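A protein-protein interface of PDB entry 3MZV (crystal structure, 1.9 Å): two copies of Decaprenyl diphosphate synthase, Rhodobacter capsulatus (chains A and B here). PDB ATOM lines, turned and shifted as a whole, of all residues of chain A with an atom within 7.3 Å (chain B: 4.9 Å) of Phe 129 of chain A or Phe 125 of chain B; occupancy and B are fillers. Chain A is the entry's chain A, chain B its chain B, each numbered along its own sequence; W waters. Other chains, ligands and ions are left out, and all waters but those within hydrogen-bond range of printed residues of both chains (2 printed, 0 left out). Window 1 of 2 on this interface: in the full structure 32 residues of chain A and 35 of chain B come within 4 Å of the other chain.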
ATOM      1  N   THR A  81      13.788  15.183 -33.155  1.00  0.00           N
ATOM      2  CA  THR A  81      13.558  13.872 -32.583  1.00  0.00           C
ATOM      3  C   THR A  81      14.526  13.577 -31.432  1.00  0.00           C
ATOM      4  O   THR A  81      14.124  13.087 -30.378  1.00  0.00           O
ATOM      5  CB  THR A  81      13.669  12.769 -33.633  1.00  0.00           C
ATOM      6  OG1 THR A  81      12.670  13.014 -34.660  1.00  0.00           O
ATOM      7  CG2 THR A  81      13.508  11.368 -32.992  1.00  0.00           C
ATOM      8  N   PHE A  84      13.504  15.593 -28.402  1.00  0.00           N
ATOM      9  CA  PHE A  84      12.339  15.028 -27.722  1.00  0.00           C
ATOM     10  C   PHE A  84      12.752  13.809 -26.884  1.00  0.00           C
ATOM     11  O   PHE A  84      12.301  13.659 -25.754  1.00  0.00           O
ATOM     12  CB  PHE A  84      11.260  14.594 -28.728  1.00  0.00           C
ATOM     13  CG  PHE A  84      10.376  15.697 -29.221  1.00  0.00           C
ATOM     14  CD1 PHE A  84       9.743  16.534 -28.336  1.00  0.00           C
ATOM     15  CD2 PHE A  84      10.075  15.823 -30.591  1.00  0.00           C
ATOM     16  CE1 PHE A  84       8.823  17.552 -28.797  1.00  0.00           C
ATOM     17  CE2 PHE A  84       9.188  16.823 -31.052  1.00  0.00           C
ATOM     18  CZ  PHE A  84       8.534  17.657 -30.133  1.00  0.00           C
ATOM     19  N   ILE A  85      13.602  12.954 -27.453  1.00  0.00           N
ATOM     20  CA  ILE A  85      14.035  11.716 -26.761  1.00  0.00           C
ATOM     21  C   ILE A  85      14.804  12.115 -25.499  1.00  0.00           C
ATOM     22  O   ILE A  85      14.596  11.516 -24.426  1.00  0.00           O
ATOM     23  CB  ILE A  85      14.874  10.770 -27.674  1.00  0.00           C
ATOM     24  CG1 ILE A  85      13.987  10.124 -28.739  1.00  0.00           C
ATOM     25  CG2 ILE A  85      15.603   9.667 -26.855  1.00  0.00           C
ATOM     26  CD1 ILE A  85      14.785   9.248 -29.756  1.00  0.00           C
ATOM     27  N   GLY A 121       6.363  12.480 -20.761  1.00  0.00           N
ATOM     28  CA  GLY A 121       7.497  11.787 -21.358  1.00  0.00           C
ATOM     29  C   GLY A 121       7.037  10.809 -22.435  1.00  0.00           C
ATOM     30  O   GLY A 121       7.650  10.757 -23.527  1.00  0.00           O
ATOM     31  N   ASP A 122       5.974  10.041 -22.130  1.00  0.00           N
ATOM     32  CA  ASP A 122       5.442   9.065 -23.074  1.00  0.00           C
ATOM     33  C   ASP A 122       4.933   9.767 -24.323  1.00  0.00           C
ATOM     34  O   ASP A 122       5.124   9.305 -25.425  1.00  0.00           O
ATOM     35  CB  ASP A 122       4.304   8.237 -22.450  1.00  0.00           C
ATOM     36  CG  ASP A 122       4.787   7.192 -21.467  1.00  0.00           C
ATOM     37  OD1 ASP A 122       6.000   6.897 -21.459  1.00  0.00           O
ATOM     38  OD2 ASP A 122       3.931   6.667 -20.730  1.00  0.00           O
ATOM     39  N   TYR A 123       4.259  10.880 -24.144  1.00  0.00           N
ATOM     40  CA  TYR A 123       3.747  11.639 -25.281  1.00  0.00           C
ATOM     41  C   TYR A 123       4.893  12.102 -26.170  1.00  0.00           C
ATOM     42  O   TYR A 123       4.847  11.931 -27.388  1.00  0.00           O
ATOM     43  CB  TYR A 123       3.003  12.881 -24.788  1.00  0.00           C
ATOM     44  CG  TYR A 123       2.248  13.629 -25.879  1.00  0.00           C
ATOM     45  CD1 TYR A 123       1.084  13.114 -26.405  1.00  0.00           C
ATOM     46  CD2 TYR A 123       2.690  14.859 -26.362  1.00  0.00           C
ATOM     47  CE1 TYR A 123       0.352  13.795 -27.375  1.00  0.00           C
ATOM     48  CE2 TYR A 123       1.939  15.565 -27.340  1.00  0.00           C
ATOM     49  CZ  TYR A 123       0.789  15.004 -27.839  1.00  0.00           C
ATOM     50  OH  TYR A 123       0.012  15.634 -28.805  1.00  0.00           O
ATOM     51  N   LEU A 124       5.954  12.580 -25.535  1.00  0.00           N
ATOM     52  CA  LEU A 124       7.120  13.073 -26.267  1.00  0.00           C
ATOM     53  C   LEU A 124       7.877  11.976 -27.020  1.00  0.00           C
ATOM     54  O   LEU A 124       8.189  12.152 -28.202  1.00  0.00           O
ATOM     55  CB  LEU A 124       8.062  13.872 -25.367  1.00  0.00           C
ATOM     56  CG  LEU A 124       7.457  15.150 -24.774  1.00  0.00           C
ATOM     57  CD1 LEU A 124       8.472  15.826 -23.878  1.00  0.00           C
ATOM     58  CD2 LEU A 124       6.887  16.137 -25.854  1.00  0.00           C
ATOM     59  N   PHE A 125       8.122  10.853 -26.364  1.00  0.00           N
ATOM     60  CA  PHE A 125       8.726   9.713 -26.990  1.00  0.00           C
ATOM     61  C   PHE A 125       7.890   9.342 -28.257  1.00  0.00           C
ATOM     62  O   PHE A 125       8.449   9.173 -29.369  1.00  0.00           O
ATOM     63  CB  PHE A 125       8.757   8.501 -26.053  1.00  0.00           C
ATOM     64  CG  PHE A 125       9.914   8.428 -25.061  1.00  0.00           C
ATOM     65  CD1 PHE A 125      11.233   8.418 -25.485  1.00  0.00           C
ATOM     66  CD2 PHE A 125       9.661   8.145 -23.703  1.00  0.00           C
ATOM     67  CE1 PHE A 125      12.317   8.240 -24.551  1.00  0.00           C
ATOM     68  CE2 PHE A 125      10.739   7.959 -22.772  1.00  0.00           C
ATOM     69  CZ  PHE A 125      12.062   8.037 -23.212  1.00  0.00           C
ATOM     70  N   ALA A 126       6.571   9.226 -28.104  1.00  0.00           N
ATOM     71  CA  ALA A 126       5.739   8.851 -29.252  1.00  0.00           C
ATOM     72  C   ALA A 126       5.762   9.891 -30.380  1.00  0.00           C
ATOM     73  O   ALA A 126       5.894   9.536 -31.545  1.00  0.00           O
ATOM     74  CB  ALA A 126       4.264   8.564 -28.829  1.00  0.00           C
ATOM     75  N   ARG A 127       5.594  11.153 -30.036  1.00  0.00           N
ATOM     76  CA  ARG A 127       5.690  12.205 -31.052  1.00  0.00           C
ATOM     77  C   ARG A 127       7.052  12.229 -31.747  1.00  0.00           C
ATOM     78  O   ARG A 127       7.097  12.520 -32.938  1.00  0.00           O
ATOM     79  CB  ARG A 127       5.372  13.559 -30.449  1.00  0.00           C
ATOM     80  CG  ARG A 127       3.906  13.698 -30.026  1.00  0.00           C
ATOM     81  CD  ARG A 127       2.957  13.551 -31.215  1.00  0.00           C
ATOM     82  NE  ARG A 127       1.596  13.924 -30.881  1.00  0.00           N
ATOM     83  CZ  ARG A 127       0.513  13.467 -31.485  1.00  0.00           C
ATOM     84  NH1 ARG A 127       0.602  12.617 -32.510  1.00  0.00           N
ATOM     85  NH2 ARG A 127      -0.680  13.861 -31.060  1.00  0.00           N
ATOM     86  N   SER A 128       8.126  11.892 -31.027  1.00  0.00           N
ATOM     87  CA  SER A 128       9.441  11.810 -31.637  1.00  0.00           C
ATOM     88  C   SER A 128       9.514  10.717 -32.684  1.00  0.00           C
ATOM     89  O   SER A 128      10.077  10.908 -33.752  1.00  0.00           O
ATOM     90  CB  SER A 128      10.535  11.664 -30.586  1.00  0.00           C
ATOM     91  OG  SER A 128      10.795  10.322 -30.219  1.00  0.00           O
ATOM     92  N   PHE A 129       8.909   9.579 -32.410  1.00  0.00           N
ATOM     93  CA  PHE A 129       8.949   8.471 -33.336  1.00  0.00           C
ATOM     94  C   PHE A 129       8.065   8.830 -34.535  1.00  0.00           C
ATOM     95  O   PHE A 129       8.383   8.540 -35.686  1.00  0.00           O
ATOM     96  CB  PHE A 129       8.563   7.137 -32.600  1.00  0.00           C
ATOM     97  CG  PHE A 129       9.623   6.621 -31.571  1.00  0.00           C
ATOM     98  CD1 PHE A 129      10.836   7.228 -31.385  1.00  0.00           C
ATOM     99  CD2 PHE A 129       9.337   5.467 -30.796  1.00  0.00           C
ATOM    100  CE1 PHE A 129      11.794   6.720 -30.478  1.00  0.00           C
ATOM    101  CE2 PHE A 129      10.292   4.956 -29.871  1.00  0.00           C
ATOM    102  CZ  PHE A 129      11.515   5.597 -29.728  1.00  0.00           C
ATOM    103  N   GLN A 130       6.939   9.488 -34.297  1.00  0.00           N
ATOM    104  CA  GLN A 130       6.052   9.854 -35.371  1.00  0.00           C
ATOM    105  C   GLN A 130       6.743  10.878 -36.293  1.00  0.00           C
ATOM    106  O   GLN A 130       6.652  10.806 -37.533  1.00  0.00           O
ATOM    107  CB  GLN A 130       4.691  10.383 -34.809  1.00  0.00           C
ATOM    108  CG  GLN A 130       3.837  11.082 -35.831  1.00  0.00           C
ATOM    109  CD  GLN A 130       2.623  11.830 -35.232  1.00  0.00           C
ATOM    110  OE1 GLN A 130       2.703  12.412 -34.153  1.00  0.00           O
ATOM    111  NE2 GLN A 130       1.504  11.794 -35.938  1.00  0.00           N
ATOM    112  N   LEU A 131       7.491  11.779 -35.680  1.00  0.00           N
ATOM    113  CA  LEU A 131       8.227  12.852 -36.433  1.00  0.00           C
ATOM    114  C   LEU A 131       9.324  12.265 -37.345  1.00  0.00           C
ATOM    115  O   LEU A 131       9.398  12.678 -38.491  1.00  0.00           O
ATOM    116  CB  LEU A 131       8.839  13.873 -35.476  1.00  0.00           C
ATOM    117  CG  LEU A 131       9.681  15.014 -36.056  1.00  0.00           C
ATOM    118  CD1 LEU A 131       8.954  15.831 -37.146  1.00  0.00           C
ATOM    119  CD2 LEU A 131      10.151  15.888 -34.924  1.00  0.00           C
ATOM    120  N   MET A 132      10.039  11.251 -36.841  1.00  0.00           N
ATOM    121  CA  MET A 132      11.186  10.551 -37.503  1.00  0.00           C
ATOM    122  C   MET A 132      10.656   9.959 -38.827  1.00  0.00           C
ATOM    123  O   MET A 132      11.385   9.843 -39.809  1.00  0.00           O
ATOM    124  CB  MET A 132      11.638   9.361 -36.593  1.00  0.00           C
ATOM    125  CG  MET A 132      13.066   9.106 -36.032  1.00  0.00           C
ATOM    126  SD  MET A 132      12.772   7.727 -34.834  1.00  0.00           S
ATOM    127  CE  MET A 132      11.882   6.338 -35.452  1.00  0.00           C
ATOM    128  N   THR A 133       9.417   9.451 -38.834  1.00  0.00           N
ATOM    129  CA  THR A 133       8.838   8.799 -40.049  1.00  0.00           C
ATOM    130  C   THR A 133       8.738   9.745 -41.256  1.00  0.00           C
ATOM    131  O   THR A 133       8.745   9.276 -42.432  1.00  0.00           O
ATOM    132  CB  THR A 133       7.457   8.141 -39.808  1.00  0.00           C
ATOM    133  OG1 THR A 133       6.431   9.130 -39.673  1.00  0.00           O
ATOM    134  CG2 THR A 133       7.482   7.200 -38.602  1.00  0.00           C
ATOM    135  N   ASP A 134       8.692  11.057 -41.006  1.00  0.00           N
ATOM    136  CA  ASP A 134       8.642  12.041 -42.096  1.00  0.00           C
ATOM    137  C   ASP A 134       9.890  11.937 -42.987  1.00  0.00           C
ATOM    138  O   ASP A 134       9.835  12.336 -44.156  1.00  0.00           O
ATOM    139  CB  ASP A 134       8.561  13.525 -41.605  1.00  0.00           C
ATOM    140  CG  ASP A 134       7.174  13.907 -41.020  1.00  0.00           C
ATOM    141  OD1 ASP A 134       6.211  13.095 -41.072  1.00  0.00           O
ATOM    142  OD2 ASP A 134       7.080  15.025 -40.433  1.00  0.00           O
ATOM    143  N   MET A 141      15.867   5.560 -38.066  1.00  0.00           N
ATOM    144  CA  MET A 141      14.797   5.283 -37.133  1.00  0.00           C
ATOM    145  C   MET A 141      15.177   4.082 -36.283  1.00  0.00           C
ATOM    146  O   MET A 141      14.921   4.080 -35.084  1.00  0.00           O
ATOM    147  CB  MET A 141      13.466   5.029 -37.854  1.00  0.00           C
ATOM    148  CG  MET A 141      12.830   6.219 -38.599  1.00  0.00           C
ATOM    149  SD  MET A 141      11.140   5.733 -39.284  1.00  0.00           S
ATOM    150  CE  MET A 141      11.477   6.291 -41.011  1.00  0.00           C
ATOM    151  N   LEU A 144      17.738   5.393 -33.675  1.00  0.00           N
ATOM    152  CA  LEU A 144      17.194   6.214 -32.605  1.00  0.00           C
ATOM    153  C   LEU A 144      16.323   5.416 -31.669  1.00  0.00           C
ATOM    154  O   LEU A 144      16.337   5.672 -30.433  1.00  0.00           O
ATOM    155  CB  LEU A 144      16.493   7.444 -33.145  1.00  0.00           C
ATOM    156  CG  LEU A 144      17.357   8.512 -33.836  1.00  0.00           C
ATOM    157  CD1 LEU A 144      16.559   9.575 -34.579  1.00  0.00           C
ATOM    158  CD2 LEU A 144      18.200   9.216 -32.818  1.00  0.00           C
ATOM    159  N   ALA A 145      15.580   4.426 -32.213  1.00  0.00           N
ATOM    160  CA  ALA A 145      14.814   3.508 -31.352  1.00  0.00           C
ATOM    161  C   ALA A 145      15.765   2.718 -30.465  1.00  0.00           C
ATOM    162  O   ALA A 145      15.509   2.508 -29.265  1.00  0.00           O
ATOM    163  CB  ALA A 145      13.907   2.554 -32.187  1.00  0.00           C
ATOM    164  N   ASN A 146      16.877   2.272 -31.054  1.00  0.00           N
ATOM    165  CA  ASN A 146      17.878   1.527 -30.301  1.00  0.00           C
ATOM    166  C   ASN A 146      18.518   2.370 -29.223  1.00  0.00           C
ATOM    167  O   ASN A 146      18.699   1.892 -28.120  1.00  0.00           O
ATOM    168  CB  ASN A 146      18.974   0.969 -31.214  1.00  0.00           C
ATOM    169  CG  ASN A 146      20.042   0.215 -30.446  1.00  0.00           C
ATOM    170  OD1 ASN A 146      19.819  -0.934 -30.090  1.00  0.00           O
ATOM    171  ND2 ASN A 146      21.235   0.841 -30.245  1.00  0.00           N
ATOM    172  N   SER A 148      17.170   4.885 -27.659  1.00  0.00           N
ATOM    173  CA  SER A 148      16.199   5.007 -26.565  1.00  0.00           C
ATOM    174  C   SER A 148      16.162   3.740 -25.705  1.00  0.00           C
ATOM    175  O   SER A 148      16.109   3.839 -24.443  1.00  0.00           O
ATOM    176  CB  SER A 148      14.834   5.404 -27.142  1.00  0.00           C
ATOM    177  OG  SER A 148      13.875   5.553 -26.073  1.00  0.00           O
ATOM    178  N   ALA A 149      16.271   2.565 -26.336  1.00  0.00           N
ATOM    179  CA  ALA A 149      16.230   1.320 -25.635  1.00  0.00           C
ATOM    180  C   ALA A 149      17.457   1.235 -24.741  1.00  0.00           C
ATOM    181  O   ALA A 149      17.382   0.778 -23.596  1.00  0.00           O
ATOM    182  CB  ALA A 149      16.237   0.123 -26.594  1.00  0.00           C
ATOM    183  N   ILE B  85       3.271  -2.120 -27.082  1.00  0.00           N
ATOM    184  CA  ILE B  85       2.717  -0.827 -26.728  1.00  0.00           C
ATOM    185  C   ILE B  85       1.677  -0.959 -25.610  1.00  0.00           C
ATOM    186  O   ILE B  85       1.689  -0.198 -24.630  1.00  0.00           O
ATOM    187  CB  ILE B  85       2.120  -0.101 -27.971  1.00  0.00           C
ATOM    188  CG1 ILE B  85       3.246   0.294 -28.939  1.00  0.00           C
ATOM    189  CG2 ILE B  85       1.347   1.118 -27.553  1.00  0.00           C
ATOM    190  CD1 ILE B  85       2.738   0.664 -30.333  1.00  0.00           C
ATOM    191  N   ALA B  88       3.619  -1.775 -22.328  1.00  0.00           N
ATOM    192  CA  ALA B  88       4.266  -0.553 -21.839  1.00  0.00           C
ATOM    193  C   ALA B  88       3.264   0.372 -21.218  1.00  0.00           C
ATOM    194  O   ALA B  88       3.554   0.938 -20.144  1.00  0.00           O
ATOM    195  CB  ALA B  88       5.048   0.208 -23.036  1.00  0.00           C
ATOM    196  N   GLY B 121       8.802  -0.293 -19.220  1.00  0.00           N
ATOM    197  CA  GLY B 121       7.864   0.156 -20.231  1.00  0.00           C
ATOM    198  C   GLY B 121       8.601   0.942 -21.322  1.00  0.00           C
ATOM    199  O   GLY B 121       8.312   0.800 -22.518  1.00  0.00           O
ATOM    200  N   ASP B 122       9.548   1.791 -20.930  1.00  0.00           N
ATOM    201  CA  ASP B 122      10.294   2.552 -21.967  1.00  0.00           C
ATOM    202  C   ASP B 122      11.121   1.625 -22.910  1.00  0.00           C
ATOM    203  O   ASP B 122      11.188   1.815 -24.145  1.00  0.00           O
ATOM    204  CB  ASP B 122      11.245   3.579 -21.321  1.00  0.00           C
ATOM    205  CG  ASP B 122      10.510   4.749 -20.642  1.00  0.00           C
ATOM    206  OD1 ASP B 122       9.352   4.968 -20.932  1.00  0.00           O
ATOM    207  OD2 ASP B 122      11.145   5.466 -19.840  1.00  0.00           O
ATOM    208  N   TYR B 123      11.794   0.662 -22.299  1.00  0.00           N
ATOM    209  CA  TYR B 123      12.550  -0.341 -23.030  1.00  0.00           C
ATOM    210  C   TYR B 123      11.693  -1.067 -24.061  1.00  0.00           C
ATOM    211  O   TYR B 123      12.115  -1.207 -25.199  1.00  0.00           O
ATOM    212  CB  TYR B 123      13.175  -1.371 -22.077  1.00  0.00           C
ATOM    213  CG  TYR B 123      14.200  -2.271 -22.760  1.00  0.00           C
ATOM    214  CD1 TYR B 123      15.456  -1.787 -23.116  1.00  0.00           C
ATOM    215  CD2 TYR B 123      13.880  -3.589 -23.110  1.00  0.00           C
ATOM    216  CE1 TYR B 123      16.406  -2.605 -23.729  1.00  0.00           C
ATOM    217  CE2 TYR B 123      14.840  -4.410 -23.719  1.00  0.00           C
ATOM    218  CZ  TYR B 123      16.074  -3.915 -24.036  1.00  0.00           C
ATOM    219  OH  TYR B 123      17.031  -4.719 -24.648  1.00  0.00           O
ATOM    220  N   LEU B 124      10.511  -1.520 -23.667  1.00  0.00           N
ATOM    221  CA  LEU B 124       9.629  -2.246 -24.564  1.00  0.00           C
ATOM    222  C   LEU B 124       9.096  -1.349 -25.684  1.00  0.00           C
ATOM    223  O   LEU B 124       8.991  -1.767 -26.837  1.00  0.00           O
ATOM    224  CB  LEU B 124       8.444  -2.822 -23.802  1.00  0.00           C
ATOM    225  CG  LEU B 124       8.857  -3.751 -22.643  1.00  0.00           C
ATOM    226  CD1 LEU B 124       7.647  -4.324 -21.972  1.00  0.00           C
ATOM    227  CD2 LEU B 124       9.797  -4.832 -23.155  1.00  0.00           C
ATOM    228  N   PHE B 125       8.735  -0.133 -25.321  1.00  0.00           N
ATOM    229  CA  PHE B 125       8.280   0.818 -26.299  1.00  0.00           C
ATOM    230  C   PHE B 125       9.357   1.042 -27.369  1.00  0.00           C
ATOM    231  O   PHE B 125       9.062   1.043 -28.550  1.00  0.00           O
ATOM    232  CB  PHE B 125       7.931   2.138 -25.631  1.00  0.00           C
ATOM    233  CG  PHE B 125       7.219   3.090 -26.567  1.00  0.00           C
ATOM    234  CD1 PHE B 125       7.855   4.227 -27.045  1.00  0.00           C
ATOM    235  CD2 PHE B 125       5.957   2.792 -27.039  1.00  0.00           C
ATOM    236  CE1 PHE B 125       7.203   5.109 -27.929  1.00  0.00           C
ATOM    237  CE2 PHE B 125       5.299   3.653 -27.922  1.00  0.00           C
ATOM    238  CZ  PHE B 125       5.944   4.840 -28.373  1.00  0.00           C
ATOM    239  N   ALA B 126      10.575   1.291 -26.952  1.00  0.00           N
ATOM    240  CA  ALA B 126      11.695   1.496 -27.874  1.00  0.00           C
ATOM    241  C   ALA B 126      11.960   0.275 -28.768  1.00  0.00           C
ATOM    242  O   ALA B 126      12.090   0.387 -29.984  1.00  0.00           O
ATOM    243  CB  ALA B 126      12.969   1.859 -27.089  1.00  0.00           C
ATOM    244  N   ARG B 127      12.042  -0.896 -28.148  1.00  0.00           N
ATOM    245  CA  ARG B 127      12.255  -2.114 -28.880  1.00  0.00           C
ATOM    246  C   ARG B 127      11.138  -2.364 -29.897  1.00  0.00           C
ATOM    247  O   ARG B 127      11.391  -2.902 -30.965  1.00  0.00           O
ATOM    248  CB  ARG B 127      12.338  -3.282 -27.891  1.00  0.00           C
ATOM    249  CG  ARG B 127      13.615  -3.233 -27.023  1.00  0.00           C
ATOM    250  CD  ARG B 127      14.829  -4.035 -27.480  1.00  0.00           C
ATOM    251  NE  ARG B 127      15.779  -3.221 -28.197  1.00  0.00           N
ATOM    252  CZ  ARG B 127      17.094  -3.049 -27.973  1.00  0.00           C
ATOM    253  NH1 ARG B 127      17.727  -2.238 -28.789  1.00  0.00           N
ATOM    254  NH2 ARG B 127      17.811  -3.642 -27.014  1.00  0.00           N
ATOM    255  N   SER B 128       9.932  -1.985 -29.556  1.00  0.00           N
ATOM    256  CA  SER B 128       8.839  -2.193 -30.465  1.00  0.00           C
ATOM    257  C   SER B 128       8.973  -1.325 -31.705  1.00  0.00           C
ATOM    258  O   SER B 128       8.654  -1.785 -32.800  1.00  0.00           O
ATOM    259  CB  SER B 128       7.496  -2.018 -29.780  1.00  0.00           C
ATOM    260  OG  SER B 128       7.051  -0.677 -29.678  1.00  0.00           O
ATOM    261  N   PHE B 129       9.415  -0.071 -31.546  1.00  0.00           N
ATOM    262  CA  PHE B 129       9.671   0.738 -32.728  1.00  0.00           C
ATOM    263  C   PHE B 129      10.876   0.282 -33.525  1.00  0.00           C
ATOM    264  O   PHE B 129      10.853   0.337 -34.731  1.00  0.00           O
ATOM    265  CB  PHE B 129       9.631   2.226 -32.404  1.00  0.00           C
ATOM    266  CG  PHE B 129       8.246   2.706 -32.364  1.00  0.00           C
ATOM    267  CD1 PHE B 129       7.483   2.467 -31.254  1.00  0.00           C
ATOM    268  CD2 PHE B 129       7.638   3.253 -33.519  1.00  0.00           C
ATOM    269  CE1 PHE B 129       6.163   2.837 -31.219  1.00  0.00           C
ATOM    270  CE2 PHE B 129       6.335   3.630 -33.481  1.00  0.00           C
ATOM    271  CZ  PHE B 129       5.590   3.408 -32.317  1.00  0.00           C
ATOM    272  N   ALA B 145       2.904   5.124 -33.880  1.00  0.00           N
ATOM    273  CA  ALA B 145       3.462   6.220 -33.089  1.00  0.00           C
ATOM    274  C   ALA B 145       2.398   7.193 -32.654  1.00  0.00           C
ATOM    275  O   ALA B 145       2.324   7.617 -31.485  1.00  0.00           O
ATOM    276  CB  ALA B 145       4.614   6.967 -33.891  1.00  0.00           C
ATOM    277  N   SER B 148       0.240   5.835 -29.959  1.00  0.00           N
ATOM    278  CA  SER B 148       0.936   5.856 -28.685  1.00  0.00           C
ATOM    279  C   SER B 148       0.841   7.206 -28.052  1.00  0.00           C
ATOM    280  O   SER B 148       0.631   7.303 -26.828  1.00  0.00           O
ATOM    281  CB  SER B 148       2.363   5.402 -28.845  1.00  0.00           C
ATOM    282  OG  SER B 148       2.413   4.070 -29.326  1.00  0.00           O
HETATM  283  O   HOH W   1      11.583   4.543 -25.111  1.00  0.00           O
HETATM  284  O   HOH W   2      20.857  -2.608 -27.926  1.00  0.00           O
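OD1 of Asp 122 of chain A touches OD1 of Asp 122 of chain B (3.9 Å).
Asp 122 of chain B touches Phe 125 of chain A (OD1 to CE2, 3.8 Å).
Ala 145 of chain B touches Ala 126 of chain A (O to CB, 3.4 Å).
Phe 125 of chain B touches Phe 129 of chain A (CE1 to CD2, 3.6 Å).
Phe 129 of chain A touches Ala 145 of chain B (C to CB, 3.97 Å).
CB of Ala 145 of chain B touches N of Gln 130 of chain A (3.5 Å).
Ala 126 of chain B touches Ala 145 of chain A.
Ala 126 of chain B touches Ser 148 of chain A.
Ala 149 of chain A touches Tyr 123 of chain B (O to CD1, 3.2 Å).
CB of Ala 149 of chain A touches NH1 of Arg 127 of chain B, at 3.6 Å.
Phe 129 of chain A touches three residues of chain B.
Of the printed residues of chain A, Phe 125 of chain B touches Phe 129.
Of the printed residues of chain B, Asp 122 of chain A touches Asp 122 (3.9 Å).
Printed residues of chain A within 4 Å of Ala 126 of chain B: Ala 145, Ser 148 and Ala 149.
Of the printed residues of chain A, Tyr 123 of chain B touches Ala 149.
Printed residues of chain A within 4 Å of Ser 148 of chain B: Ala 126.
Of the printed residues of chain B, Phe 125 of chain A touches Asp 122.
Leu 124 of chain A touches none of the printed residues of chain B.
Gly 121 of chain B touches none of the printed residues of chain A.
The nearest printed residue of chain A that does not touch Ser 148 of chain B is Asp 122 of chain A (5.1 Å).
Hydrophobic or aromatic side chains of chain B within 4 Å of the printed part of chain A: Tyr 123, Phe 125, Ala 126, Phe 129 and Ala 145.
Of the 23 printed residues of chain A, 9 touch a printed residue of chain B.
Hydrophobic or aromatic side chains of chain A within 4 Å of the printed part of chain B: Phe 125, Ala 126, Phe 129, Ala 145 and Ala 149.
Among the printed residues, 14 pairs touch across the chains.
The backbone carbonyl oxygen (O) of Phe 125 of chain A lies within hydrogen-bond range of the side-chain hydroxyl (OG) of Ser 128 of chain A.
NH1 of Arg 127 of chain A is in hydrogen-bond range of OE1 of Gln 130 of chain A (2.7 Å).
OG1 of Thr 133 of chain A lies within hydrogen-bond range of O of Gln 130 of chain A, 2.7 Å away.
The guanidinium group (NH2) of Arg 127 of chain B is in hydrogen-bond range of the side-chain hydroxyl (OH) of Tyr 123 of chain B (2.7 Å).
The backbone carbonyl oxygen (O) of Phe 125 of chain B is in hydrogen-bond range of the side-chain hydroxyl (OG) of Ser 128 of chain B (2.9 Å).
Phe 125 of chain A touches Asp 122 of chain B, but with the chains exchanged Asp 122 of chain A does not touch Phe 125 of chain B (5.3 Å).
Ala 126 of chain A touches Ala 145 of chain B, and with the chains exchanged Ala 145 of chain A touches Ala 126 of chain B.
Ala 126 of chain A touches Ser 148 of chain B, and with the chains exchanged Ser 148 of chain A touches Ala 126 of chain B.
Phe 129 of chain A touches Phe 125 of chain B, but with the chains exchanged Phe 125 of chain A does not touch Phe 129 of chain B (7.0 Å).
Of the 14 pairs that touch across the chains among the printed residues, 6 have their exchanged pair printed and touching as well.
The side-chain amide oxygen (OD1) of Asn 146 of chain A lies within hydrogen-bond range of the guanidinium group (NH1) of Arg 127 of chain B (2.8 Å).
Water W1 lies within hydrogen-bond range of OG of Ser 148 of chain A and O of Asp 122 of chain B.
Water W2 bridges the side-chain amide oxygen (OD1) of Asn 146 of chain A (2.9 Å) and the guanidinium group (NH1) of Arg 127 of chain B (3.3 Å).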
